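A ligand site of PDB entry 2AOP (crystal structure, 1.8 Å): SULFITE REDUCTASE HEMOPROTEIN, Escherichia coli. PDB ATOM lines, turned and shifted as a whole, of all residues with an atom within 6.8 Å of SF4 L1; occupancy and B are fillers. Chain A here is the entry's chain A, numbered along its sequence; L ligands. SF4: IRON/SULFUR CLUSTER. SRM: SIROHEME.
The backbone NH of Cys 410 is in hydrogen-bond range of the side-chain hydroxyl of Thr 404 (3.3 Å). SG of Cys 406 lies close to ND2 of Asn 408 (3.5 Å). SG of Cys 361 lies close to N of Ser 363 (3.7 Å). The backbone NH of Cys 361 lies within hydrogen-bond range of the backbone carbonyl oxygen of Val 403. SG of Cys 367 sits close to N of Leu 369, 3.4 Å away. The side-chain hydroxyl of Thr 404 is in hydrogen-bond range of the backbone NH of Gly 411 (3.1 Å). The backbone carbonyl oxygen (O) of Gly 405 lies within hydrogen-bond range of the backbone NH (N) of Met 371 (3.0 Å). OG of Ser 363 is in hydrogen-bond range of O of Ala 372 (2.7 Å).
Leu 369 touches SF4 L1. CA of Ala 370 touches S4 of SF4 L1, 3.5 Å away. Gly 405 touches SF4 L1 (CA to S4, 3.6 Å). Hydrophobic or aromatic side chains that line SF4 L1: Leu 369 and Ala 370. Within 4 Å of SF4 L1: Cys 361, Ser 363, Cys 367, Leu 369, Ala 370, Thr 404, Gly 405, Cys 406, Asn 408, Gly 409 and Cys 410. The nearest printed residue that does not touch SF4 L1 is Val 362 (4.04 Å).
S2 of SF4 L1 lies close to N of Cys 410, 3.4 Å away. The side-chain sulfur (SG) of Cys 410 is bound to an iron atom (FE4) of SF4 L1 (2.2 Å). The backbone NH (N) of Cys 406 sits close to a sulfur (S2) of SF4 L1 (3.7 Å). The side-chain sulfur (SG) of Cys 406 binds an iron atom (FE3) of SF4 L1 (2.2 Å). SG of Cys 361 binds FE1 of SF4 L1. An iron atom (FE2) of SF4 L1 is bound by the side-chain sulfur of Cys 367 (2.3 Å). A sulfur (S2) of SF4 L1 lies close to the side-chain hydroxyl of Thr 404, 3.1 Å away. ND2 of Asn 408 lies close to S1 of SF4 L1, 3.5 Å away. A sulfur (S3) of SF4 L1 sits close to the backbone NH of Ser 363, 3.6 Å away. The backbone NH (N) of Gly 409 sits close to a sulfur (S2) of SF4 L1 (3.8 Å). SG of Cys 410 is bound to FE of SRM L2, 2.7 Å away. The backbone NH of Cys 367 sits at hydrogen-bond distance from an oxygen (O1A) of SRM L2, 3.4 Å away. O3B of SRM L2 is in hydrogen-bond range of N of Val 362, 3.1 Å away.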
ATOM      1  N   ALA A 360     -14.034 -21.611  29.506  1.00  0.00           N
ATOM      2  CA  ALA A 360     -13.227 -20.435  29.222  1.00  0.00           C
ATOM      3  C   ALA A 360     -13.927 -19.626  28.121  1.00  0.00           C
ATOM      4  O   ALA A 360     -14.783 -20.158  27.395  1.00  0.00           O
ATOM      5  CB  ALA A 360     -11.833 -20.837  28.768  1.00  0.00           C
ATOM      6  N   CYS A 361     -13.626 -18.333  28.072  1.00  0.00           N
ATOM      7  CA  CYS A 361     -14.178 -17.480  27.035  1.00  0.00           C
ATOM      8  C   CYS A 361     -13.241 -17.559  25.819  1.00  0.00           C
ATOM      9  O   CYS A 361     -12.144 -18.107  25.895  1.00  0.00           O
ATOM     10  CB  CYS A 361     -14.245 -16.035  27.495  1.00  0.00           C
ATOM     11  SG  CYS A 361     -12.589 -15.295  27.665  1.00  0.00           S
ATOM     12  N   VAL A 362     -13.671 -16.979  24.708  1.00  0.00           N
ATOM     13  CA  VAL A 362     -12.891 -16.955  23.483  1.00  0.00           C
ATOM     14  C   VAL A 362     -11.491 -16.310  23.660  1.00  0.00           C
ATOM     15  O   VAL A 362     -10.459 -16.944  23.360  1.00  0.00           O
ATOM     16  CB  VAL A 362     -13.634 -16.212  22.392  1.00  0.00           C
ATOM     17  CG1 VAL A 362     -12.777 -16.122  21.143  1.00  0.00           C
ATOM     18  CG2 VAL A 362     -14.918 -16.944  22.069  1.00  0.00           C
ATOM     19  N   SER A 363     -11.465 -15.059  24.134  1.00  0.00           N
ATOM     20  CA  SER A 363     -10.199 -14.321  24.334  1.00  0.00           C
ATOM     21  C   SER A 363      -9.377 -14.277  23.029  1.00  0.00           C
ATOM     22  O   SER A 363      -9.954 -14.165  21.942  1.00  0.00           O
ATOM     23  CB  SER A 363      -9.389 -14.955  25.477  1.00  0.00           C
ATOM     24  OG  SER A 363      -8.217 -14.203  25.762  1.00  0.00           O
ATOM     25  N   PHE A 364      -8.044 -14.335  23.145  1.00  0.00           N
ATOM     26  CA  PHE A 364      -7.174 -14.314  21.970  1.00  0.00           C
ATOM     27  C   PHE A 364      -7.472 -15.550  21.120  1.00  0.00           C
ATOM     28  O   PHE A 364      -7.777 -16.609  21.669  1.00  0.00           O
ATOM     29  CB  PHE A 364      -5.705 -14.348  22.370  1.00  0.00           C
ATOM     30  CG  PHE A 364      -5.271 -13.172  23.177  1.00  0.00           C
ATOM     31  CD1 PHE A 364      -5.204 -11.897  22.613  1.00  0.00           C
ATOM     32  CD2 PHE A 364      -4.909 -13.333  24.522  1.00  0.00           C
ATOM     33  CE1 PHE A 364      -4.767 -10.805  23.365  1.00  0.00           C
ATOM     34  CE2 PHE A 364      -4.480 -12.245  25.288  1.00  0.00           C
ATOM     35  CZ  PHE A 364      -4.415 -10.982  24.712  1.00  0.00           C
ATOM     36  N   CYS A 367     -10.553 -11.817  20.328  1.00  0.00           N
ATOM     37  CA  CYS A 367     -11.104 -10.767  21.179  1.00  0.00           C
ATOM     38  C   CYS A 367     -10.211  -9.559  21.332  1.00  0.00           C
ATOM     39  O   CYS A 367      -9.098  -9.655  21.839  1.00  0.00           O
ATOM     40  CB  CYS A 367     -11.461 -11.304  22.556  1.00  0.00           C
ATOM     41  SG  CYS A 367     -12.373 -10.051  23.484  1.00  0.00           S
ATOM     42  N   PRO A 368     -10.725  -8.372  20.997  1.00  0.00           N
ATOM     43  CA  PRO A 368      -9.915  -7.162  21.119  1.00  0.00           C
ATOM     44  C   PRO A 368      -9.717  -6.643  22.552  1.00  0.00           C
ATOM     45  O   PRO A 368      -8.896  -5.760  22.802  1.00  0.00           O
ATOM     46  CB  PRO A 368     -10.688  -6.173  20.245  1.00  0.00           C
ATOM     47  CG  PRO A 368     -12.117  -6.596  20.457  1.00  0.00           C
ATOM     48  CD  PRO A 368     -12.031  -8.093  20.375  1.00  0.00           C
ATOM     49  N   LEU A 369     -10.460  -7.206  23.497  1.00  0.00           N
ATOM     50  CA  LEU A 369     -10.381  -6.761  24.883  1.00  0.00           C
ATOM     51  C   LEU A 369      -9.608  -7.726  25.748  1.00  0.00           C
ATOM     52  O   LEU A 369      -9.394  -7.462  26.924  1.00  0.00           O
ATOM     53  CB  LEU A 369     -11.796  -6.633  25.431  1.00  0.00           C
ATOM     54  CG  LEU A 369     -12.776  -5.847  24.552  1.00  0.00           C
ATOM     55  CD1 LEU A 369     -14.136  -5.829  25.183  1.00  0.00           C
ATOM     56  CD2 LEU A 369     -12.273  -4.423  24.337  1.00  0.00           C
ATOM     57  N   ALA A 370      -9.131  -8.801  25.132  1.00  0.00           N
ATOM     58  CA  ALA A 370      -8.420  -9.830  25.863  1.00  0.00           C
ATOM     59  C   ALA A 370      -7.159  -9.373  26.596  1.00  0.00           C
ATOM     60  O   ALA A 370      -6.356  -8.631  26.063  1.00  0.00           O
ATOM     61  CB  ALA A 370      -8.089 -10.966  24.918  1.00  0.00           C
ATOM     62  N   MET A 371      -7.010  -9.816  27.852  1.00  0.00           N
ATOM     63  CA  MET A 371      -5.836  -9.488  28.627  1.00  0.00           C
ATOM     64  C   MET A 371      -4.934 -10.722  28.763  1.00  0.00           C
ATOM     65  O   MET A 371      -3.714 -10.604  28.664  1.00  0.00           O
ATOM     66  CB  MET A 371      -6.224  -8.940  30.001  1.00  0.00           C
ATOM     67  CG  MET A 371      -6.949  -7.595  29.948  1.00  0.00           C
ATOM     68  SD  MET A 371      -7.496  -7.083  31.591  1.00  0.00           S
ATOM     69  CE  MET A 371      -8.115  -5.422  31.283  1.00  0.00           C
ATOM     70  N   ALA A 372      -5.525 -11.899  28.946  1.00  0.00           N
ATOM     71  CA  ALA A 372      -4.763 -13.136  29.074  1.00  0.00           C
ATOM     72  C   ALA A 372      -5.499 -14.205  28.285  1.00  0.00           C
ATOM     73  O   ALA A 372      -6.707 -14.078  28.050  1.00  0.00           O
ATOM     74  CB  ALA A 372      -4.640 -13.533  30.532  1.00  0.00           C
ATOM     75  N   ALA A 374      -7.506 -17.554  27.312  1.00  0.00           N
ATOM     76  CA  ALA A 374      -8.555 -18.262  28.028  1.00  0.00           C
ATOM     77  C   ALA A 374      -8.837 -19.566  27.283  1.00  0.00           C
ATOM     78  O   ALA A 374      -8.395 -20.629  27.718  1.00  0.00           O
ATOM     79  CB  ALA A 374      -9.812 -17.409  28.144  1.00  0.00           C
ATOM     80  N   VAL A 403     -12.152 -19.878  33.358  1.00  0.00           N
ATOM     81  CA  VAL A 403     -11.136 -18.893  33.050  1.00  0.00           C
ATOM     82  C   VAL A 403     -11.754 -17.872  32.116  1.00  0.00           C
ATOM     83  O   VAL A 403     -12.360 -18.213  31.104  1.00  0.00           O
ATOM     84  CB  VAL A 403      -9.948 -19.546  32.345  1.00  0.00           C
ATOM     85  CG1 VAL A 403      -8.846 -18.538  32.091  1.00  0.00           C
ATOM     86  CG2 VAL A 403      -9.428 -20.723  33.180  1.00  0.00           C
ATOM     87  N   THR A 404     -11.638 -16.610  32.489  1.00  0.00           N
ATOM     88  CA  THR A 404     -12.159 -15.539  31.674  1.00  0.00           C
ATOM     89  C   THR A 404     -10.960 -14.635  31.312  1.00  0.00           C
ATOM     90  O   THR A 404     -10.080 -14.381  32.146  1.00  0.00           O
ATOM     91  CB  THR A 404     -13.323 -14.814  32.400  1.00  0.00           C
ATOM     92  OG1 THR A 404     -14.078 -14.055  31.446  1.00  0.00           O
ATOM     93  CG2 THR A 404     -12.835 -13.915  33.532  1.00  0.00           C
ATOM     94  N   GLY A 405     -10.867 -14.284  30.032  1.00  0.00           N
ATOM     95  CA  GLY A 405      -9.750 -13.494  29.516  1.00  0.00           C
ATOM     96  C   GLY A 405      -9.538 -12.083  30.020  1.00  0.00           C
ATOM     97  O   GLY A 405      -8.438 -11.536  29.906  1.00  0.00           O
ATOM     98  N   CYS A 406     -10.591 -11.463  30.535  1.00  0.00           N
ATOM     99  CA  CYS A 406     -10.482 -10.124  31.072  1.00  0.00           C
ATOM    100  C   CYS A 406     -11.662 -10.008  32.022  1.00  0.00           C
ATOM    101  O   CYS A 406     -12.550 -10.872  32.009  1.00  0.00           O
ATOM    102  CB  CYS A 406     -10.510  -9.077  29.941  1.00  0.00           C
ATOM    103  SG  CYS A 406     -12.122  -8.683  29.209  1.00  0.00           S
ATOM    104  N   PRO A 407     -11.713  -8.945  32.832  1.00  0.00           N
ATOM    105  CA  PRO A 407     -12.809  -8.799  33.795  1.00  0.00           C
ATOM    106  C   PRO A 407     -14.227  -8.612  33.272  1.00  0.00           C
ATOM    107  O   PRO A 407     -15.165  -8.585  34.057  1.00  0.00           O
ATOM    108  CB  PRO A 407     -12.332  -7.653  34.678  1.00  0.00           C
ATOM    109  CG  PRO A 407     -11.598  -6.794  33.731  1.00  0.00           C
ATOM    110  CD  PRO A 407     -10.793  -7.801  32.921  1.00  0.00           C
ATOM    111  N   ASN A 408     -14.393  -8.494  31.951  1.00  0.00           N
ATOM    112  CA  ASN A 408     -15.731  -8.380  31.375  1.00  0.00           C
ATOM    113  C   ASN A 408     -16.503  -9.633  31.788  1.00  0.00           C
ATOM    114  O   ASN A 408     -17.731  -9.626  31.873  1.00  0.00           O
ATOM    115  CB  ASN A 408     -15.669  -8.224  29.865  1.00  0.00           C
ATOM    116  CG  ASN A 408     -15.342  -6.809  29.450  1.00  0.00           C
ATOM    117  OD1 ASN A 408     -15.607  -5.867  30.202  1.00  0.00           O
ATOM    118  ND2 ASN A 408     -14.758  -6.634  28.282  1.00  0.00           N
ATOM    119  N   GLY A 409     -15.764 -10.718  32.020  1.00  0.00           N
ATOM    120  CA  GLY A 409     -16.331 -11.946  32.537  1.00  0.00           C
ATOM    121  C   GLY A 409     -17.123 -12.932  31.727  1.00  0.00           C
ATOM    122  O   GLY A 409     -17.832 -13.752  32.321  1.00  0.00           O
ATOM    123  N   CYS A 410     -16.949 -12.932  30.402  1.00  0.00           N
ATOM    124  CA  CYS A 410     -17.677 -13.838  29.522  1.00  0.00           C
ATOM    125  C   CYS A 410     -17.562 -15.338  29.873  1.00  0.00           C
ATOM    126  O   CYS A 410     -18.505 -16.099  29.656  1.00  0.00           O
ATOM    127  CB  CYS A 410     -17.238 -13.619  28.081  1.00  0.00           C
ATOM    128  SG  CYS A 410     -17.154 -11.864  27.646  1.00  0.00           S
ATOM    129  N   GLY A 411     -16.417 -15.727  30.418  1.00  0.00           N
ATOM    130  CA  GLY A 411     -16.219 -17.120  30.803  1.00  0.00           C
ATOM    131  C   GLY A 411     -16.961 -17.516  32.063  1.00  0.00           C
ATOM    132  O   GLY A 411     -16.903 -18.679  32.471  1.00  0.00           O
HETATM  133 FE1  SF4 L   1     -12.919 -13.127  27.268  1.00  0.00          FE
HETATM  134 FE2  SF4 L   1     -12.930 -11.110  25.413  1.00  0.00          FE
HETATM  135 FE3  SF4 L   1     -12.738 -10.457  28.042  1.00  0.00          FE
HETATM  136 FE4  SF4 L   1     -15.082 -11.567  27.032  1.00  0.00          FE
HETATM  137  S1  SF4 L   1     -14.231  -9.612  26.490  1.00  0.00           S
HETATM  138  S2  SF4 L   1     -13.905 -12.048  29.045  1.00  0.00           S
HETATM  139  S3  SF4 L   1     -14.206 -13.033  25.416  1.00  0.00           S
HETATM  140  S4  SF4 L   1     -11.268 -11.695  26.787  1.00  0.00           S
HETATM  141 FE   SRM L   2     -19.327 -11.410  26.119  1.00  0.00          FE
HETATM  142  CHA SRM L   2     -17.900  -8.425  25.076  1.00  0.00           C
HETATM  143  CHB SRM L   2     -17.678 -13.111  23.696  1.00  0.00           C
HETATM  144  CHC SRM L   2     -20.930 -14.287  27.108  1.00  0.00           C
HETATM  145  CHD SRM L   2     -19.922 -10.032  29.210  1.00  0.00           C
HETATM  146  NA  SRM L   2     -18.058 -10.871  24.604  1.00  0.00           N
HETATM  147  C1A SRM L   2     -17.668  -9.492  24.311  1.00  0.00           C
HETATM  148  C2A SRM L   2     -17.126  -9.631  22.881  1.00  0.00           C
HETATM  149  CMA SRM L   2     -18.160  -9.528  21.808  1.00  0.00           C
HETATM  150  CDA SRM L   2     -15.928  -8.635  22.728  1.00  0.00           C
HETATM  151  CEA SRM L   2     -16.224  -7.245  22.209  1.00  0.00           C
HETATM  152  O3A SRM L   2     -16.921  -6.474  22.889  1.00  0.00           O
HETATM  153  O4A SRM L   2     -15.767  -6.930  21.089  1.00  0.00           O
HETATM  154  C3A SRM L   2     -16.327 -10.909  23.064  1.00  0.00           C
HETATM  155  CAA SRM L   2     -16.082 -11.497  21.679  1.00  0.00           C
HETATM  156  CBA SRM L   2     -14.919 -12.468  21.652  1.00  0.00           C
HETATM  157  CCA SRM L   2     -14.741 -13.161  20.314  1.00  0.00           C
HETATM  158  O1A SRM L   2     -13.732 -12.894  19.635  1.00  0.00           O
HETATM  159  O2A SRM L   2     -15.598 -13.991  19.944  1.00  0.00           O
HETATM  160  C4A SRM L   2     -17.391 -11.742  23.771  1.00  0.00           C
HETATM  161  NB  SRM L   2     -19.303 -13.386  25.555  1.00  0.00           N
HETATM  162  C1B SRM L   2     -18.567 -13.851  24.505  1.00  0.00           C
HETATM  163  C2B SRM L   2     -18.659 -15.391  24.480  1.00  0.00           C
HETATM  164  CMB SRM L   2     -18.506 -15.843  22.954  1.00  0.00           C
HETATM  165  CDB SRM L   2     -17.642 -16.145  25.413  1.00  0.00           C
HETATM  166  CEB SRM L   2     -17.597 -17.630  25.153  1.00  0.00           C
HETATM  167  O3B SRM L   2     -16.485 -18.156  25.040  1.00  0.00           O
HETATM  168  O4B SRM L   2     -18.659 -18.270  25.055  1.00  0.00           O
HETATM  169  C3B SRM L   2     -20.184 -15.439  24.910  1.00  0.00           C
HETATM  170  CAB SRM L   2     -21.070 -14.944  23.792  1.00  0.00           C
HETATM  171  CBB SRM L   2     -22.447 -15.118  24.352  1.00  0.00           C
HETATM  172  CCB SRM L   2     -23.519 -14.809  23.353  1.00  0.00           C
HETATM  173  O1B SRM L   2     -23.833 -15.681  22.523  1.00  0.00           O
HETATM  174  O2B SRM L   2     -24.059 -13.695  23.390  1.00  0.00           O
HETATM  175  C4B SRM L   2     -20.171 -14.386  26.018  1.00  0.00           C
HETATM  176  NC  SRM L   2     -20.284 -12.016  27.845  1.00  0.00           N
HETATM  177  C1C SRM L   2     -20.919 -13.216  28.001  1.00  0.00           C
HETATM  178  C2C SRM L   2     -21.145 -13.377  29.404  1.00  0.00           C
HETATM  179  CDC SRM L   2     -21.722 -14.704  30.021  1.00  0.00           C
HETATM  180  CEC SRM L   2     -23.206 -14.904  29.772  1.00  0.00           C
HETATM  181  O3C SRM L   2     -23.872 -13.982  29.259  1.00  0.00           O
HETATM  182  O4C SRM L   2     -23.726 -15.991  30.068  1.00  0.00           O
HETATM  183  C3C SRM L   2     -20.905 -12.133  30.050  1.00  0.00           C
HETATM  184  CAC SRM L   2     -20.877 -11.973  31.486  1.00  0.00           C
HETATM  185  CBC SRM L   2     -22.268 -11.721  32.083  1.00  0.00           C
HETATM  186  CCC SRM L   2     -22.646 -10.252  32.055  1.00  0.00           C
HETATM  187  O1C SRM L   2     -22.999  -9.755  30.978  1.00  0.00           O
HETATM  188  O2C SRM L   2     -22.586  -9.602  33.103  1.00  0.00           O
HETATM  189  C4C SRM L   2     -20.275 -11.355  29.069  1.00  0.00           C
HETATM  190  ND  SRM L   2     -19.088  -9.582  26.861  1.00  0.00           N
HETATM  191  C1D SRM L   2     -19.507  -9.206  28.161  1.00  0.00           C
HETATM  192  C2D SRM L   2     -19.093  -7.806  28.362  1.00  0.00           C
HETATM  193  CAD SRM L   2     -19.165  -6.995  29.660  1.00  0.00           C
HETATM  194  CBD SRM L   2     -20.612  -6.557  29.716  1.00  0.00           C
HETATM  195  CCD SRM L   2     -20.892  -5.545  30.787  1.00  0.00           C
HETATM  196  O1D SRM L   2     -22.068  -5.439  31.201  1.00  0.00           O
HETATM  197  O2D SRM L   2     -19.960  -4.831  31.210  1.00  0.00           O
HETATM  198  C3D SRM L   2     -18.533  -7.422  27.186  1.00  0.00           C
HETATM  199  CDD SRM L   2     -17.876  -6.083  26.843  1.00  0.00           C
HETATM  200  CED SRM L   2     -18.905  -5.013  26.511  1.00  0.00           C
HETATM  201  O3D SRM L   2     -20.039  -5.357  26.131  1.00  0.00           O
HETATM  202  O4D SRM L   2     -18.578  -3.824  26.612  1.00  0.00           O
HETATM  203  C4D SRM L   2     -18.498  -8.500  26.284  1.00  0.00           C
